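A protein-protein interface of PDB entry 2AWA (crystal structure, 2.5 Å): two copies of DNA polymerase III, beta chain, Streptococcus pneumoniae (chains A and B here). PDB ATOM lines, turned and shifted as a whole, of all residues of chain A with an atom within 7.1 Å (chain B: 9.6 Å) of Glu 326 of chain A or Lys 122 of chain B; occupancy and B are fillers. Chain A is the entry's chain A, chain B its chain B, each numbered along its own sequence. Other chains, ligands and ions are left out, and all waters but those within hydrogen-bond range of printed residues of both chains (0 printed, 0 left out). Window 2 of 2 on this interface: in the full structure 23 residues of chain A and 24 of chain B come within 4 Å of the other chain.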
ATOM      1  N   SER A 286     -12.310  28.035   4.547  1.00  0.00           N
ATOM      2  CA  SER A 286     -13.510  28.886   4.452  1.00  0.00           C
ATOM      3  C   SER A 286     -13.218  30.158   3.655  1.00  0.00           C
ATOM      4  O   SER A 286     -14.043  30.601   2.862  1.00  0.00           O
ATOM      5  CB  SER A 286     -14.052  29.273   5.824  1.00  0.00           C
ATOM      6  OG  SER A 286     -14.071  28.163   6.682  1.00  0.00           O
ATOM      7  N   ARG A 289     -13.117  29.367  -0.089  1.00  0.00           N
ATOM      8  CA  ARG A 289     -14.489  29.296  -0.610  1.00  0.00           C
ATOM      9  C   ARG A 289     -15.068  30.711  -0.773  1.00  0.00           C
ATOM     10  O   ARG A 289     -15.614  31.061  -1.820  1.00  0.00           O
ATOM     11  CB  ARG A 289     -15.385  28.446   0.310  1.00  0.00           C
ATOM     12  CG  ARG A 289     -15.201  26.951   0.115  1.00  0.00           C
ATOM     13  CD  ARG A 289     -16.252  26.122   0.851  1.00  0.00           C
ATOM     14  NE  ARG A 289     -16.029  26.111   2.296  1.00  0.00           N
ATOM     15  CZ  ARG A 289     -15.087  25.401   2.908  1.00  0.00           C
ATOM     16  NH1 ARG A 289     -14.280  24.610   2.220  1.00  0.00           N
ATOM     17  NH2 ARG A 289     -14.956  25.461   4.225  1.00  0.00           N
ATOM     18  N   VAL A 310     -21.129  33.015  17.605  1.00  0.00           N
ATOM     19  CA  VAL A 310     -21.265  32.459  16.268  1.00  0.00           C
ATOM     20  C   VAL A 310     -20.550  33.332  15.247  1.00  0.00           C
ATOM     21  O   VAL A 310     -20.779  34.546  15.177  1.00  0.00           O
ATOM     22  CB  VAL A 310     -22.744  32.327  15.855  1.00  0.00           C
ATOM     23  CG1 VAL A 310     -22.879  31.399  14.649  1.00  0.00           C
ATOM     24  CG2 VAL A 310     -23.608  31.829  17.036  1.00  0.00           C
ATOM     25  N   VAL A 311     -19.684  32.700  14.459  1.00  0.00           N
ATOM     26  CA  VAL A 311     -18.960  33.379  13.407  1.00  0.00           C
ATOM     27  C   VAL A 311     -19.416  32.849  12.054  1.00  0.00           C
ATOM     28  O   VAL A 311     -19.553  31.641  11.853  1.00  0.00           O
ATOM     29  CB  VAL A 311     -17.450  33.180  13.569  1.00  0.00           C
ATOM     30  CG1 VAL A 311     -16.683  33.929  12.490  1.00  0.00           C
ATOM     31  CG2 VAL A 311     -17.014  33.638  14.957  1.00  0.00           C
ATOM     32  N   SER A 312     -19.653  33.764  11.127  1.00  0.00           N
ATOM     33  CA  SER A 312     -20.137  33.402   9.814  1.00  0.00           C
ATOM     34  C   SER A 312     -19.549  34.293   8.729  1.00  0.00           C
ATOM     35  O   SER A 312     -19.237  35.464   8.978  1.00  0.00           O
ATOM     36  CB  SER A 312     -21.660  33.461   9.795  1.00  0.00           C
ATOM     37  OG  SER A 312     -22.111  34.791   9.889  1.00  0.00           O
ATOM     38  N   ALA A 313     -19.395  33.733   7.529  1.00  0.00           N
ATOM     39  CA  ALA A 313     -18.807  34.453   6.413  1.00  0.00           C
ATOM     40  C   ALA A 313     -19.821  34.612   5.302  1.00  0.00           C
ATOM     41  O   ALA A 313     -20.589  33.680   5.015  1.00  0.00           O
ATOM     42  CB  ALA A 313     -17.611  33.716   5.916  1.00  0.00           C
ATOM     43  N   HIS A 314     -19.821  35.791   4.674  1.00  0.00           N
ATOM     44  CA  HIS A 314     -20.827  36.140   3.652  1.00  0.00           C
ATOM     45  C   HIS A 314     -20.206  36.850   2.466  1.00  0.00           C
ATOM     46  O   HIS A 314     -19.341  37.713   2.632  1.00  0.00           O
ATOM     47  CB  HIS A 314     -21.914  37.023   4.259  1.00  0.00           C
ATOM     48  CG  HIS A 314     -22.511  36.453   5.508  1.00  0.00           C
ATOM     49  ND1 HIS A 314     -23.522  35.518   5.488  1.00  0.00           N
ATOM     50  CD2 HIS A 314     -22.192  36.639   6.812  1.00  0.00           C
ATOM     51  CE1 HIS A 314     -23.822  35.173   6.728  1.00  0.00           C
ATOM     52  NE2 HIS A 314     -23.030  35.838   7.550  1.00  0.00           N
ATOM     53  N   ASN A 324     -22.700  31.614   2.216  1.00  0.00           N
ATOM     54  CA  ASN A 324     -23.144  31.774   3.597  1.00  0.00           C
ATOM     55  C   ASN A 324     -22.573  30.599   4.394  1.00  0.00           C
ATOM     56  O   ASN A 324     -23.081  29.480   4.328  1.00  0.00           O
ATOM     57  CB  ASN A 324     -24.677  31.816   3.647  1.00  0.00           C
ATOM     58  CG  ASN A 324     -25.232  31.917   5.060  1.00  0.00           C
ATOM     59  OD1 ASN A 324     -24.508  32.139   6.033  1.00  0.00           O
ATOM     60  ND2 ASN A 324     -26.539  31.750   5.172  1.00  0.00           N
ATOM     61  N   GLU A 325     -21.492  30.851   5.115  1.00  0.00           N
ATOM     62  CA  GLU A 325     -20.793  29.805   5.841  1.00  0.00           C
ATOM     63  C   GLU A 325     -20.698  30.113   7.343  1.00  0.00           C
ATOM     64  O   GLU A 325     -20.392  31.232   7.736  1.00  0.00           O
ATOM     65  CB  GLU A 325     -19.404  29.600   5.242  1.00  0.00           C
ATOM     66  CG  GLU A 325     -18.688  28.391   5.802  1.00  0.00           C
ATOM     67  CD  GLU A 325     -17.469  27.957   5.010  1.00  0.00           C
ATOM     68  OE1 GLU A 325     -17.284  28.377   3.852  1.00  0.00           O
ATOM     69  OE2 GLU A 325     -16.684  27.168   5.562  1.00  0.00           O
ATOM     70  N   GLU A 326     -21.023  29.112   8.165  1.00  0.00           N
ATOM     71  CA  GLU A 326     -20.767  29.148   9.600  1.00  0.00           C
ATOM     72  C   GLU A 326     -19.404  28.523   9.821  1.00  0.00           C
ATOM     73  O   GLU A 326     -19.194  27.369   9.463  1.00  0.00           O
ATOM     74  CB  GLU A 326     -21.837  28.368  10.359  1.00  0.00           C
ATOM     75  CG  GLU A 326     -21.646  28.380  11.882  1.00  0.00           C
ATOM     76  CD  GLU A 326     -22.856  27.850  12.651  1.00  0.00           C
ATOM     77  OE1 GLU A 326     -23.994  28.287  12.372  1.00  0.00           O
ATOM     78  OE2 GLU A 326     -22.665  27.005  13.548  1.00  0.00           O
ATOM     79  N   ILE A 327     -18.481  29.304  10.377  1.00  0.00           N
ATOM     80  CA  ILE A 327     -17.101  28.872  10.613  1.00  0.00           C
ATOM     81  C   ILE A 327     -16.958  28.450  12.058  1.00  0.00           C
ATOM     82  O   ILE A 327     -17.233  29.237  12.963  1.00  0.00           O
ATOM     83  CB  ILE A 327     -16.098  30.034  10.358  1.00  0.00           C
ATOM     84  CG1 ILE A 327     -16.159  30.476   8.890  1.00  0.00           C
ATOM     85  CG2 ILE A 327     -14.656  29.646  10.772  1.00  0.00           C
ATOM     86  CD1 ILE A 327     -15.700  31.880   8.673  1.00  0.00           C
ATOM     87  N   ASP A 328     -16.517  27.209  12.272  1.00  0.00           N
ATOM     88  CA  ASP A 328     -16.271  26.703  13.622  1.00  0.00           C
ATOM     89  C   ASP A 328     -15.098  27.460  14.243  1.00  0.00           C
ATOM     90  O   ASP A 328     -14.137  27.829  13.579  1.00  0.00           O
ATOM     91  CB  ASP A 328     -16.054  25.187  13.640  1.00  0.00           C
ATOM     92  CG  ASP A 328     -17.368  24.404  13.772  1.00  0.00           C
ATOM     93  N   LEU B 101     -15.677  22.516  -1.775  1.00  0.00           N
ATOM     94  CA  LEU B 101     -16.562  22.215  -0.650  1.00  0.00           C
ATOM     95  C   LEU B 101     -15.881  21.303   0.374  1.00  0.00           C
ATOM     96  O   LEU B 101     -15.060  20.467  -0.001  1.00  0.00           O
ATOM     97  CB  LEU B 101     -17.866  21.584  -1.148  1.00  0.00           C
ATOM     98  CG  LEU B 101     -18.686  22.516  -2.049  1.00  0.00           C
ATOM     99  CD1 LEU B 101     -19.855  21.789  -2.721  1.00  0.00           C
ATOM    100  CD2 LEU B 101     -19.183  23.743  -1.273  1.00  0.00           C
ATOM    101  N   PRO B 102     -16.207  21.471   1.674  1.00  0.00           N
ATOM    102  CA  PRO B 102     -15.455  20.790   2.732  1.00  0.00           C
ATOM    103  C   PRO B 102     -15.812  19.330   3.004  1.00  0.00           C
ATOM    104  O   PRO B 102     -14.928  18.576   3.391  1.00  0.00           O
ATOM    105  CB  PRO B 102     -15.745  21.646   3.968  1.00  0.00           C
ATOM    106  CG  PRO B 102     -17.068  22.223   3.734  1.00  0.00           C
ATOM    107  CD  PRO B 102     -17.273  22.325   2.235  1.00  0.00           C
ATOM    108  N   ASP B 103     -17.068  18.931   2.795  1.00  0.00           N
ATOM    109  CA  ASP B 103     -17.566  17.605   3.236  1.00  0.00           C
ATOM    110  C   ASP B 103     -17.635  16.549   2.125  1.00  0.00           C
ATOM    111  O   ASP B 103     -17.623  16.869   0.937  1.00  0.00           O
ATOM    112  CB  ASP B 103     -18.946  17.744   3.904  1.00  0.00           C
ATOM    113  CG  ASP B 103     -18.856  18.118   5.407  1.00  0.00           C
ATOM    114  OD1 ASP B 103     -17.836  18.712   5.848  1.00  0.00           O
ATOM    115  OD2 ASP B 103     -19.824  17.807   6.154  1.00  0.00           O
ATOM    116  N   THR B 105     -20.108  14.488   1.242  1.00  0.00           N
ATOM    117  CA  THR B 105     -21.331  14.541   0.451  1.00  0.00           C
ATOM    118  C   THR B 105     -21.779  15.979   0.323  1.00  0.00           C
ATOM    119  O   THR B 105     -21.299  16.866   1.044  1.00  0.00           O
ATOM    120  CB  THR B 105     -22.501  13.739   1.089  1.00  0.00           C
ATOM    121  OG1 THR B 105     -22.905  14.336   2.335  1.00  0.00           O
ATOM    122  CG2 THR B 105     -22.112  12.274   1.318  1.00  0.00           C
ATOM    123  N   LEU B 118     -25.867  24.992  -2.996  1.00  0.00           N
ATOM    124  CA  LEU B 118     -25.002  23.853  -2.689  1.00  0.00           C
ATOM    125  C   LEU B 118     -24.687  23.845  -1.206  1.00  0.00           C
ATOM    126  O   LEU B 118     -23.942  24.677  -0.733  1.00  0.00           O
ATOM    127  CB  LEU B 118     -23.699  23.932  -3.490  1.00  0.00           C
ATOM    128  CG  LEU B 118     -23.847  23.883  -5.016  1.00  0.00           C
ATOM    129  CD1 LEU B 118     -22.573  24.322  -5.700  1.00  0.00           C
ATOM    130  CD2 LEU B 118     -24.248  22.507  -5.492  1.00  0.00           C
ATOM    131  N   THR B 119     -25.248  22.900  -0.466  1.00  0.00           N
ATOM    132  CA  THR B 119     -24.929  22.787   0.956  1.00  0.00           C
ATOM    133  C   THR B 119     -23.975  21.621   1.182  1.00  0.00           C
ATOM    134  O   THR B 119     -24.210  20.501   0.709  1.00  0.00           O
ATOM    135  CB  THR B 119     -26.187  22.629   1.825  1.00  0.00           C
ATOM    136  OG1 THR B 119     -27.174  23.580   1.405  1.00  0.00           O
ATOM    137  CG2 THR B 119     -25.853  22.864   3.302  1.00  0.00           C
ATOM    138  N   SER B 120     -22.890  21.913   1.890  1.00  0.00           N
ATOM    139  CA  SER B 120     -21.870  20.941   2.197  1.00  0.00           C
ATOM    140  C   SER B 120     -21.263  21.331   3.527  1.00  0.00           C
ATOM    141  O   SER B 120     -20.436  22.233   3.599  1.00  0.00           O
ATOM    142  CB  SER B 120     -20.811  20.945   1.114  1.00  0.00           C
ATOM    143  OG  SER B 120     -19.728  20.118   1.469  1.00  0.00           O
ATOM    144  N   GLY B 121     -21.681  20.651   4.581  1.00  0.00           N
ATOM    145  CA  GLY B 121     -21.270  20.993   5.919  1.00  0.00           C
ATOM    146  C   GLY B 121     -21.967  22.255   6.380  1.00  0.00           C
ATOM    147  O   GLY B 121     -23.177  22.404   6.216  1.00  0.00           O
ATOM    148  N   LYS B 122     -21.194  23.169   6.950  1.00  0.00           N
ATOM    149  CA  LYS B 122     -21.715  24.450   7.396  1.00  0.00           C
ATOM    150  C   LYS B 122     -21.541  25.500   6.302  1.00  0.00           C
ATOM    151  O   LYS B 122     -21.715  26.682   6.534  1.00  0.00           O
ATOM    152  CB  LYS B 122     -21.003  24.871   8.681  1.00  0.00           C
ATOM    153  CG  LYS B 122     -21.172  23.865   9.816  1.00  0.00           C
ATOM    154  CD  LYS B 122     -21.129  24.522  11.190  1.00  0.00           C
ATOM    155  CE  LYS B 122     -21.698  23.613  12.282  1.00  0.00           C
ATOM    156  N   SER B 123     -21.212  25.048   5.099  1.00  0.00           N
ATOM    157  CA  SER B 123     -20.928  25.941   3.988  1.00  0.00           C
ATOM    158  C   SER B 123     -22.056  25.868   2.952  1.00  0.00           C
ATOM    159  O   SER B 123     -22.322  24.805   2.392  1.00  0.00           O
ATOM    160  CB  SER B 123     -19.578  25.572   3.368  1.00  0.00           C
ATOM    161  OG  SER B 123     -19.351  26.299   2.179  1.00  0.00           O
ATOM    162  N   GLU B 124     -22.732  27.000   2.740  1.00  0.00           N
ATOM    163  CA  GLU B 124     -23.823  27.102   1.759  1.00  0.00           C
ATOM    164  C   GLU B 124     -23.400  28.043   0.627  1.00  0.00           C
ATOM    165  O   GLU B 124     -22.933  29.160   0.877  1.00  0.00           O
ATOM    166  CB  GLU B 124     -25.094  27.621   2.426  1.00  0.00           C
ATOM    167  CG  GLU B 124     -26.352  27.589   1.549  1.00  0.00           C
ATOM    168  CD  GLU B 124     -27.549  28.236   2.236  1.00  0.00           C
ATOM    169  OE1 GLU B 124     -27.495  29.458   2.522  1.00  0.00           O
ATOM    170  OE2 GLU B 124     -28.542  27.520   2.511  1.00  0.00           O
ATOM    171  N   ILE B 125     -23.546  27.574  -0.607  1.00  0.00           N
ATOM    172  CA  ILE B 125     -23.108  28.316  -1.775  1.00  0.00           C
ATOM    173  C   ILE B 125     -24.157  28.217  -2.881  1.00  0.00           C
ATOM    174  O   ILE B 125     -24.475  27.121  -3.373  1.00  0.00           O
ATOM    175  CB  ILE B 125     -21.730  27.842  -2.314  1.00  0.00           C
ATOM    176  CG1 ILE B 125     -20.656  27.974  -1.238  1.00  0.00           C
ATOM    177  CG2 ILE B 125     -21.320  28.670  -3.543  1.00  0.00           C
ATOM    178  CD1 ILE B 125     -19.239  27.819  -1.757  1.00  0.00           C
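No position is printed for both chains.
Among the printed residues, pairs that only touch across the chains: Glu 325 of chain A with Lys 122 of chain B (3.3 Å), Arg 289 of chain A with Pro 102 of chain B (3.7 Å), Asn 324 of chain A with Lys 122 of chain B (3.8 Å) and Asn 324 of chain A with Ser 123 of chain B (3.999 Å).
Of the printed residues of chain B, Arg 289 of chain A touches Pro 102 and Ser 123. Val 310 of chain A touches none of the printed residues of chain B. Glu 325 of chain A touches just these residues of chain B: Lys 122 (3.3 Å) and Ser 123 (3.4 Å). Of chain B, only Lys 122 comes within 4 Å of Glu 326 of chain A. No residue of chain B comes within 4 Å of Ile 327 of chain A. Lys 122 of chain B touches just these residues of chain A: Asn 324, Glu 325 and Glu 326. Of the printed residues of chain A, Ser 123 of chain B touches Arg 289 (3.3 Å), Asn 324 (3.999 Å) and Glu 325 (3.4 Å). The nearest residue of chain B that does not touch Glu 326 of chain A is Ser 123 of chain B (5.1 Å).
The guanidinium group of Arg 289 of chain A lies within hydrogen-bond range of the side-chain hydroxyl of Ser 123 of chain B, 3.3 Å away. The side-chain carboxylate (OE1) of Glu 325 of chain A is in hydrogen-bond range of the side-chain hydroxyl (OG) of Ser 123 of chain B, at 3.4 Å. The backbone carbonyl oxygen (O) of Glu 124 of chain B sits at hydrogen-bond distance from the backbone NH (N) of Asn 324 of chain A (2.8 Å). The backbone NH of Glu 326 of chain A is in hydrogen-bond range of the backbone carbonyl oxygen of Lys 122 of chain B.
Hydrophobic or aromatic side chains of chain B within 4 Å of the printed part of chain A: Pro 102.
The backbone NH (N) of Ala 313 of chain A sits at hydrogen-bond distance from the backbone carbonyl oxygen (O) of Glu 325 of chain A (2.7 Å). The side-chain hydroxyl of Ser 286 of chain A lies within hydrogen-bond range of the side-chain carboxylate of Glu 325 of chain A (3.0 Å). OE2 of Glu 325 of chain A is in salt-bridge range of NH2 of Arg 289 of chain A (2.8 Å).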
